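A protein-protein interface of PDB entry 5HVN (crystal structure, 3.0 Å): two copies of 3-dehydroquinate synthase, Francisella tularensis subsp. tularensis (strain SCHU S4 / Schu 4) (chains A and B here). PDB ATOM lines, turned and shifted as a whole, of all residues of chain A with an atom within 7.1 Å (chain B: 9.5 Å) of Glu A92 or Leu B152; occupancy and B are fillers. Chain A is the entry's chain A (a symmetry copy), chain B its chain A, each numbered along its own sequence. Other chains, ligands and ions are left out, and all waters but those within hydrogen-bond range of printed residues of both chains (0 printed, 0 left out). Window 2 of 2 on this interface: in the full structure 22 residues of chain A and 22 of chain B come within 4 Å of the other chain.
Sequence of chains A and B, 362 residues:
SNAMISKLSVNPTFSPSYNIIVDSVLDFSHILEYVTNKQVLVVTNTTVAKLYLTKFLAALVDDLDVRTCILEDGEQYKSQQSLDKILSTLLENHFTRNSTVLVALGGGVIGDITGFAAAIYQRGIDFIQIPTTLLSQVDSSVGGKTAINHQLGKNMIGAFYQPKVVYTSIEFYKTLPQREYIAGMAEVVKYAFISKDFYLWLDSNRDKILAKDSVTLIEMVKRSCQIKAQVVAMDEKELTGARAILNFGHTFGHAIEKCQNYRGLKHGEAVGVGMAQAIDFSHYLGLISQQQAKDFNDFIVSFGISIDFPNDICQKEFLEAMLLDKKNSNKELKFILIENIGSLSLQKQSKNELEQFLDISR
Among the printed residues, 7 pairs touch across the chains. Among the printed residues, no Asp or Glu carboxylate lies within 4 Å of a Lys or Arg side-chain nitrogen of the other chain.
The backbone NH (N) of Ile B148 is in hydrogen-bond range of the backbone carbonyl oxygen (O) of Ile B157, 2.8 Å away. The backbone NH (N) of Leu B152 sits at hydrogen-bond distance from a ring nitrogen (ND1) of His B150, at 3.0 Å. O of Leu A90 is in hydrogen-bond range of OH of Tyr A121, 3.4 Å away. NE2 of His A94 lies close to O of Glu A92 (3.5 Å). The side-chain hydroxyl of Tyr A121 sits at hydrogen-bond distance from the backbone carbonyl oxygen of Phe A95, at 2.9 Å.
Glu A92 touches one residue of chain B. Of chain A, only Leu A91 (3.7 Å) and Glu A92 (3.5 Å) come within 4 Å of Leu B152. Printed residues of chain B within 4 Å of Leu A91: His B150 (3.3 Å), Leu B152 (3.7 Å) and Met B156 (3.7 Å). No residue of chain B comes within 4 Å of Asn A93. Printed residues of chain A within 4 Å of Ile B157: Leu A87. Printed residues of chain B within 4 Å of Tyr A121: Met B156 (3.7 Å). Printed residues of chain B within 4 Å of Leu A87: Ile B157 (3.5 Å). Gln B151 touches none of the printed residues of chain A. The nearest residue of chain A that does not touch Leu B152 is Ser A88 (4.3 Å).
No position is printed for both chains. Of the 7 pairs that touch across the chains among the printed residues, none has its exchanged pair printed and touching as well.
Among the printed residues, merely in contact across the chains: Leu A91 with His B150 (3.3 Å), Glu A92 with Leu B152 (3.5 Å), Leu A87 with Ile B157 (3.5 Å), Leu A91 with Met B156 (3.7 Å), Ser A88 with His B150 (3.7 Å), Tyr A121 with Met B156 (3.7 Å) and Leu A91 with Leu B152 (3.7 Å).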
ATOM      1  N   ARG A  67     -11.744  20.576   8.534  1.00  0.00           N
ATOM      2  CA  ARG A  67     -12.394  21.759   9.105  1.00  0.00           C
ATOM      3  C   ARG A  67     -11.844  23.039   8.551  1.00  0.00           C
ATOM      4  O   ARG A  67     -10.755  23.047   7.967  1.00  0.00           O
ATOM      5  CB  ARG A  67     -12.373  21.745  10.616  1.00  0.00           C
ATOM      6  CG  ARG A  67     -13.415  20.793  11.081  1.00  0.00           C
ATOM      7  CD  ARG A  67     -13.629  20.821  12.552  1.00  0.00           C
ATOM      8  NE  ARG A  67     -14.854  20.084  12.852  1.00  0.00           N
ATOM      9  CZ  ARG A  67     -14.937  18.761  12.967  1.00  0.00           C
ATOM     10  NH1 ARG A  67     -16.108  18.207  13.244  1.00  0.00           N
ATOM     11  NH2 ARG A  67     -13.864  17.991  12.806  1.00  0.00           N
ATOM     12  N   LYS A  85      -8.518  32.186  17.238  1.00  0.00           N
ATOM     13  CA  LYS A  85      -9.587  31.508  16.486  1.00  0.00           C
ATOM     14  C   LYS A  85      -9.044  30.213  15.912  1.00  0.00           C
ATOM     15  O   LYS A  85      -9.707  29.172  15.988  1.00  0.00           O
ATOM     16  CB  LYS A  85     -10.155  32.368  15.351  1.00  0.00           C
ATOM     17  CG  LYS A  85     -10.825  33.632  15.834  1.00  0.00           C
ATOM     18  CD  LYS A  85     -11.509  34.428  14.737  1.00  0.00           C
ATOM     19  CE  LYS A  85     -12.077  35.709  15.346  1.00  0.00           C
ATOM     20  NZ  LYS A  85     -12.765  36.559  14.345  1.00  0.00           N
ATOM     21  N   LEU A  87      -6.436  28.529  17.011  1.00  0.00           N
ATOM     22  CA  LEU A  87      -6.145  27.662  18.132  1.00  0.00           C
ATOM     23  C   LEU A  87      -7.405  27.050  18.786  1.00  0.00           C
ATOM     24  O   LEU A  87      -7.378  25.887  19.206  1.00  0.00           O
ATOM     25  CB  LEU A  87      -5.262  28.377  19.149  1.00  0.00           C
ATOM     26  CG  LEU A  87      -3.863  28.719  18.669  1.00  0.00           C
ATOM     27  CD1 LEU A  87      -3.183  29.538  19.742  1.00  0.00           C
ATOM     28  CD2 LEU A  87      -3.049  27.478  18.321  1.00  0.00           C
ATOM     29  N   SER A  88      -8.490  27.816  18.889  1.00  0.00           N
ATOM     30  CA  SER A  88      -9.716  27.258  19.463  1.00  0.00           C
ATOM     31  C   SER A  88     -10.284  26.193  18.554  1.00  0.00           C
ATOM     32  O   SER A  88     -10.728  25.152  19.035  1.00  0.00           O
ATOM     33  CB  SER A  88     -10.770  28.312  19.705  1.00  0.00           C
ATOM     34  OG  SER A  88     -10.318  29.187  20.691  1.00  0.00           O
ATOM     35  N   THR A  89     -10.250  26.439  17.244  1.00  0.00           N
ATOM     36  CA  THR A  89     -10.763  25.478  16.292  1.00  0.00           C
ATOM     37  C   THR A  89     -10.014  24.164  16.444  1.00  0.00           C
ATOM     38  O   THR A  89     -10.635  23.092  16.465  1.00  0.00           O
ATOM     39  CB  THR A  89     -10.732  26.019  14.860  1.00  0.00           C
ATOM     40  OG1 THR A  89     -11.654  27.107  14.769  1.00  0.00           O
ATOM     41  CG2 THR A  89     -11.165  24.957  13.872  1.00  0.00           C
ATOM     42  N   LEU A  90      -8.696  24.247  16.603  1.00  0.00           N
ATOM     43  CA  LEU A  90      -7.889  23.049  16.796  1.00  0.00           C
ATOM     44  C   LEU A  90      -8.214  22.301  18.116  1.00  0.00           C
ATOM     45  O   LEU A  90      -8.288  21.063  18.137  1.00  0.00           O
ATOM     46  CB  LEU A  90      -6.396  23.378  16.710  1.00  0.00           C
ATOM     47  CG  LEU A  90      -5.821  23.829  15.368  1.00  0.00           C
ATOM     48  CD1 LEU A  90      -4.382  24.305  15.535  1.00  0.00           C
ATOM     49  CD2 LEU A  90      -5.902  22.728  14.319  1.00  0.00           C
ATOM     50  N   LEU A  91      -8.427  23.053  19.194  1.00  0.00           N
ATOM     51  CA  LEU A  91      -8.708  22.463  20.489  1.00  0.00           C
ATOM     52  C   LEU A  91     -10.146  21.974  20.620  1.00  0.00           C
ATOM     53  O   LEU A  91     -10.378  20.877  21.151  1.00  0.00           O
ATOM     54  CB  LEU A  91      -8.318  23.418  21.613  1.00  0.00           C
ATOM     55  CG  LEU A  91      -6.827  23.773  21.714  1.00  0.00           C
ATOM     56  CD1 LEU A  91      -6.626  24.963  22.636  1.00  0.00           C
ATOM     57  CD2 LEU A  91      -5.956  22.598  22.145  1.00  0.00           C
ATOM     58  N   GLU A  92     -11.106  22.768  20.139  1.00  0.00           N
ATOM     59  CA  GLU A  92     -12.520  22.375  20.179  1.00  0.00           C
ATOM     60  C   GLU A  92     -12.742  21.084  19.436  1.00  0.00           C
ATOM     61  O   GLU A  92     -13.559  20.266  19.839  1.00  0.00           O
ATOM     62  CB  GLU A  92     -13.423  23.446  19.592  1.00  0.00           C
ATOM     63  CG  GLU A  92     -13.625  24.644  20.499  1.00  0.00           C
ATOM     64  CD  GLU A  92     -14.313  25.813  19.810  1.00  0.00           C
ATOM     65  OE1 GLU A  92     -14.463  25.793  18.564  1.00  0.00           O
ATOM     66  OE2 GLU A  92     -14.683  26.775  20.516  1.00  0.00           O
ATOM     67  N   ASN A  93     -11.997  20.885  18.368  1.00  0.00           N
ATOM     68  CA  ASN A  93     -12.143  19.682  17.577  1.00  0.00           C
ATOM     69  C   ASN A  93     -11.115  18.617  17.837  1.00  0.00           C
ATOM     70  O   ASN A  93     -10.910  17.736  17.019  1.00  0.00           O
ATOM     71  CB  ASN A  93     -12.186  20.047  16.111  1.00  0.00           C
ATOM     72  CG  ASN A  93     -13.382  20.873  15.783  1.00  0.00           C
ATOM     73  OD1 ASN A  93     -14.526  20.409  15.909  1.00  0.00           O
ATOM     74  ND2 ASN A  93     -13.140  22.111  15.340  1.00  0.00           N
ATOM     75  N   HIS A  94     -10.466  18.709  18.984  1.00  0.00           N
ATOM     76  CA  HIS A  94      -9.481  17.724  19.433  1.00  0.00           C
ATOM     77  C   HIS A  94      -8.472  17.261  18.369  1.00  0.00           C
ATOM     78  O   HIS A  94      -8.290  16.064  18.147  1.00  0.00           O
ATOM     79  CB  HIS A  94     -10.210  16.544  20.091  1.00  0.00           C
ATOM     80  CG  HIS A  94     -11.254  16.977  21.076  1.00  0.00           C
ATOM     81  ND1 HIS A  94     -11.011  17.078  22.431  1.00  0.00           N
ATOM     82  CD2 HIS A  94     -12.533  17.391  20.890  1.00  0.00           C
ATOM     83  CE1 HIS A  94     -12.101  17.508  23.039  1.00  0.00           C
ATOM     84  NE2 HIS A  94     -13.036  17.713  22.127  1.00  0.00           N
ATOM     85  N   PHE A  95      -7.840  18.224  17.711  1.00  0.00           N
ATOM     86  CA  PHE A  95      -6.796  17.947  16.744  1.00  0.00           C
ATOM     87  C   PHE A  95      -5.493  17.570  17.478  1.00  0.00           C
ATOM     88  O   PHE A  95      -4.817  18.438  18.047  1.00  0.00           O
ATOM     89  CB  PHE A  95      -6.591  19.173  15.852  1.00  0.00           C
ATOM     90  CG  PHE A  95      -7.554  19.269  14.698  1.00  0.00           C
ATOM     91  CD1 PHE A  95      -8.933  19.281  14.902  1.00  0.00           C
ATOM     92  CD2 PHE A  95      -7.071  19.414  13.398  1.00  0.00           C
ATOM     93  CE1 PHE A  95      -9.809  19.369  13.824  1.00  0.00           C
ATOM     94  CE2 PHE A  95      -7.942  19.518  12.322  1.00  0.00           C
ATOM     95  CZ  PHE A  95      -9.317  19.490  12.533  1.00  0.00           C
ATOM     96  N   TYR A 121       1.229  25.141  18.019  1.00  0.00           N
ATOM     97  CA  TYR A 121       0.209  24.163  18.399  1.00  0.00           C
ATOM     98  C   TYR A 121       0.887  22.849  18.766  1.00  0.00           C
ATOM     99  O   TYR A 121       1.449  22.164  17.913  1.00  0.00           O
ATOM    100  CB  TYR A 121      -0.815  23.942  17.295  1.00  0.00           C
ATOM    101  CG  TYR A 121      -1.953  23.121  17.810  1.00  0.00           C
ATOM    102  CD1 TYR A 121      -2.849  23.672  18.723  1.00  0.00           C
ATOM    103  CD2 TYR A 121      -2.139  21.794  17.421  1.00  0.00           C
ATOM    104  CE1 TYR A 121      -3.896  22.938  19.235  1.00  0.00           C
ATOM    105  CE2 TYR A 121      -3.199  21.057  17.927  1.00  0.00           C
ATOM    106  CZ  TYR A 121      -4.063  21.649  18.837  1.00  0.00           C
ATOM    107  OH  TYR A 121      -5.117  20.989  19.355  1.00  0.00           O
ATOM    108  N   ILE B 148       2.316  27.340  27.326  1.00  0.00           N
ATOM    109  CA  ILE B 148       1.321  28.135  28.053  1.00  0.00           C
ATOM    110  C   ILE B 148       0.003  27.380  27.985  1.00  0.00           C
ATOM    111  O   ILE B 148      -0.188  26.518  27.120  1.00  0.00           O
ATOM    112  CB  ILE B 148       1.109  29.572  27.525  1.00  0.00           C
ATOM    113  CG1 ILE B 148       0.613  29.570  26.087  1.00  0.00           C
ATOM    114  CG2 ILE B 148       2.375  30.398  27.663  1.00  0.00           C
ATOM    115  CD1 ILE B 148      -0.047  30.873  25.705  1.00  0.00           C
ATOM    116  N   ASN B 149      -0.906  27.692  28.888  1.00  0.00           N
ATOM    117  CA  ASN B 149      -2.201  27.029  28.893  1.00  0.00           C
ATOM    118  C   ASN B 149      -3.219  27.768  28.055  1.00  0.00           C
ATOM    119  O   ASN B 149      -3.064  28.956  27.751  1.00  0.00           O
ATOM    120  CB  ASN B 149      -2.740  26.927  30.320  1.00  0.00           C
ATOM    121  CG  ASN B 149      -1.869  26.092  31.216  1.00  0.00           C
ATOM    122  OD1 ASN B 149      -1.159  25.206  30.758  1.00  0.00           O
ATOM    123  ND2 ASN B 149      -1.924  26.364  32.509  1.00  0.00           N
ATOM    124  N   HIS B 150      -4.265  27.048  27.690  1.00  0.00           N
ATOM    125  CA  HIS B 150      -5.379  27.597  26.950  1.00  0.00           C
ATOM    126  C   HIS B 150      -6.601  27.137  27.717  1.00  0.00           C
ATOM    127  O   HIS B 150      -6.560  26.082  28.344  1.00  0.00           O
ATOM    128  CB  HIS B 150      -5.402  27.063  25.526  1.00  0.00           C
ATOM    129  CG  HIS B 150      -6.465  27.675  24.675  1.00  0.00           C
ATOM    130  ND1 HIS B 150      -7.769  27.231  24.678  1.00  0.00           N
ATOM    131  CD2 HIS B 150      -6.417  28.696  23.791  1.00  0.00           C
ATOM    132  CE1 HIS B 150      -8.480  27.952  23.835  1.00  0.00           C
ATOM    133  NE2 HIS B 150      -7.682  28.846  23.281  1.00  0.00           N
ATOM    134  N   GLN B 151      -7.691  27.900  27.676  1.00  0.00           N
ATOM    135  CA  GLN B 151      -8.903  27.505  28.406  1.00  0.00           C
ATOM    136  C   GLN B 151      -9.331  26.057  28.060  1.00  0.00           C
ATOM    137  O   GLN B 151      -9.850  25.331  28.906  1.00  0.00           O
ATOM    138  CB  GLN B 151     -10.035  28.500  28.159  1.00  0.00           C
ATOM    139  CG  GLN B 151     -11.226  28.342  29.098  1.00  0.00           C
ATOM    140  CD  GLN B 151     -12.350  29.341  28.837  1.00  0.00           C
ATOM    141  OE1 GLN B 151     -12.460  29.931  27.752  1.00  0.00           O
ATOM    142  NE2 GLN B 151     -13.208  29.522  29.835  1.00  0.00           N
ATOM    143  N   LEU B 152      -9.038  25.636  26.834  1.00  0.00           N
ATOM    144  CA  LEU B 152      -9.401  24.311  26.347  1.00  0.00           C
ATOM    145  C   LEU B 152      -8.366  23.222  26.564  1.00  0.00           C
ATOM    146  O   LEU B 152      -8.600  22.066  26.196  1.00  0.00           O
ATOM    147  CB  LEU B 152      -9.839  24.379  24.877  1.00  0.00           C
ATOM    148  CG  LEU B 152     -11.066  25.270  24.679  1.00  0.00           C
ATOM    149  CD1 LEU B 152     -11.516  25.264  23.231  1.00  0.00           C
ATOM    150  CD2 LEU B 152     -12.177  24.781  25.591  1.00  0.00           C
ATOM    151  N   GLY B 153      -7.233  23.567  27.164  1.00  0.00           N
ATOM    152  CA  GLY B 153      -6.194  22.566  27.408  1.00  0.00           C
ATOM    153  C   GLY B 153      -4.927  23.098  28.015  1.00  0.00           C
ATOM    154  O   GLY B 153      -4.463  24.173  27.670  1.00  0.00           O
ATOM    155  N   LYS B 154      -4.354  22.344  28.932  1.00  0.00           N
ATOM    156  CA  LYS B 154      -3.117  22.781  29.557  1.00  0.00           C
ATOM    157  C   LYS B 154      -1.905  22.359  28.738  1.00  0.00           C
ATOM    158  O   LYS B 154      -1.896  21.285  28.158  1.00  0.00           O
ATOM    159  CB  LYS B 154      -3.060  22.371  31.037  1.00  0.00           C
ATOM    160  CG  LYS B 154      -4.152  23.104  31.803  1.00  0.00           C
ATOM    161  CD  LYS B 154      -3.919  23.236  33.294  1.00  0.00           C
ATOM    162  CE  LYS B 154      -4.970  24.181  33.875  1.00  0.00           C
ATOM    163  NZ  LYS B 154      -4.702  24.511  35.304  1.00  0.00           N
ATOM    164  N   ASN B 155      -0.921  23.249  28.630  1.00  0.00           N
ATOM    165  CA  ASN B 155       0.310  23.004  27.865  1.00  0.00           C
ATOM    166  C   ASN B 155       0.091  22.584  26.422  1.00  0.00           C
ATOM    167  O   ASN B 155       0.768  21.701  25.934  1.00  0.00           O
ATOM    168  CB  ASN B 155       1.232  22.003  28.587  1.00  0.00           C
ATOM    169  CG  ASN B 155       1.826  22.574  29.857  1.00  0.00           C
ATOM    170  OD1 ASN B 155       1.123  23.084  30.709  1.00  0.00           O
ATOM    171  ND2 ASN B 155       3.136  22.475  29.986  1.00  0.00           N
ATOM    172  N   MET B 156      -0.839  23.250  25.746  1.00  0.00           N
ATOM    173  CA  MET B 156      -1.212  22.938  24.362  1.00  0.00           C
ATOM    174  C   MET B 156      -0.552  23.823  23.319  1.00  0.00           C
ATOM    175  O   MET B 156      -0.568  23.524  22.127  1.00  0.00           O
ATOM    176  CB  MET B 156      -2.732  23.073  24.223  1.00  0.00           C
ATOM    177  CG  MET B 156      -3.554  21.972  24.891  1.00  0.00           C
ATOM    178  SD  MET B 156      -3.267  20.381  24.097  1.00  0.00           S
ATOM    179  CE  MET B 156      -4.669  19.454  24.743  1.00  0.00           C
ATOM    180  N   ILE B 157       0.003  24.930  23.785  1.00  0.00           N
ATOM    181  CA  ILE B 157       0.659  25.908  22.961  1.00  0.00           C
ATOM    182  C   ILE B 157       2.040  26.058  23.567  1.00  0.00           C
ATOM    183  O   ILE B 157       2.172  26.275  24.774  1.00  0.00           O
ATOM    184  CB  ILE B 157      -0.088  27.237  23.080  1.00  0.00           C
ATOM    185  CG1 ILE B 157      -1.517  27.083  22.578  1.00  0.00           C
ATOM    186  CG2 ILE B 157       0.635  28.336  22.321  1.00  0.00           C
ATOM    187  CD1 ILE B 157      -2.397  28.261  22.945  1.00  0.00           C
ATOM    188  N   LYS B 258      -6.891  16.707  36.546  1.00  0.00           N
ATOM    189  CA  LYS B 258      -8.138  16.995  35.825  1.00  0.00           C
ATOM    190  C   LYS B 258      -9.371  16.763  36.673  1.00  0.00           C
ATOM    191  O   LYS B 258     -10.292  17.551  36.631  1.00  0.00           O
ATOM    192  CB  LYS B 258      -8.276  16.242  34.508  1.00  0.00           C
ATOM    193  CG  LYS B 258      -7.501  16.872  33.383  1.00  0.00           C
ATOM    194  CD  LYS B 258      -8.079  16.497  32.027  1.00  0.00           C
ATOM    195  CE  LYS B 258      -7.665  17.538  30.984  1.00  0.00           C
ATOM    196  NZ  LYS B 258      -8.280  17.322  29.647  1.00  0.00           N
ATOM    197  N   TYR B 262      -7.256  20.851  39.088  1.00  0.00           N
ATOM    198  CA  TYR B 262      -5.941  21.428  39.383  1.00  0.00           C
ATOM    199  C   TYR B 262      -5.901  22.239  40.718  1.00  0.00           C
ATOM    200  O   TYR B 262      -5.007  23.067  40.918  1.00  0.00           O
ATOM    201  CB  TYR B 262      -5.426  22.242  38.174  1.00  0.00           C
ATOM    202  CG  TYR B 262      -5.238  21.422  36.912  1.00  0.00           C
ATOM    203  CD1 TYR B 262      -6.327  21.113  36.070  1.00  0.00           C
ATOM    204  CD2 TYR B 262      -3.967  20.963  36.546  1.00  0.00           C
ATOM    205  CE1 TYR B 262      -6.149  20.349  34.913  1.00  0.00           C
ATOM    206  CE2 TYR B 262      -3.777  20.199  35.395  1.00  0.00           C
ATOM    207  CZ  TYR B 262      -4.864  19.892  34.585  1.00  0.00           C
ATOM    208  OH  TYR B 262      -4.655  19.139  33.453  1.00  0.00           O
ATOM    209  N   LEU B 324      -9.633  10.534  27.505  1.00  0.00           N
ATOM    210  CA  LEU B 324      -9.548  11.764  26.673  1.00  0.00           C
ATOM    211  C   LEU B 324      -8.222  11.938  25.902  1.00  0.00           C
ATOM    212  O   LEU B 324      -8.230  12.452  24.776  1.00  0.00           O
ATOM    213  CB  LEU B 324      -9.861  13.049  27.476  1.00  0.00           C
ATOM    214  CG  LEU B 324     -11.245  13.337  28.098  1.00  0.00           C
ATOM    215  CD1 LEU B 324     -11.211  14.652  28.876  1.00  0.00           C
ATOM    216  CD2 LEU B 324     -12.386  13.345  27.079  1.00  0.00           C
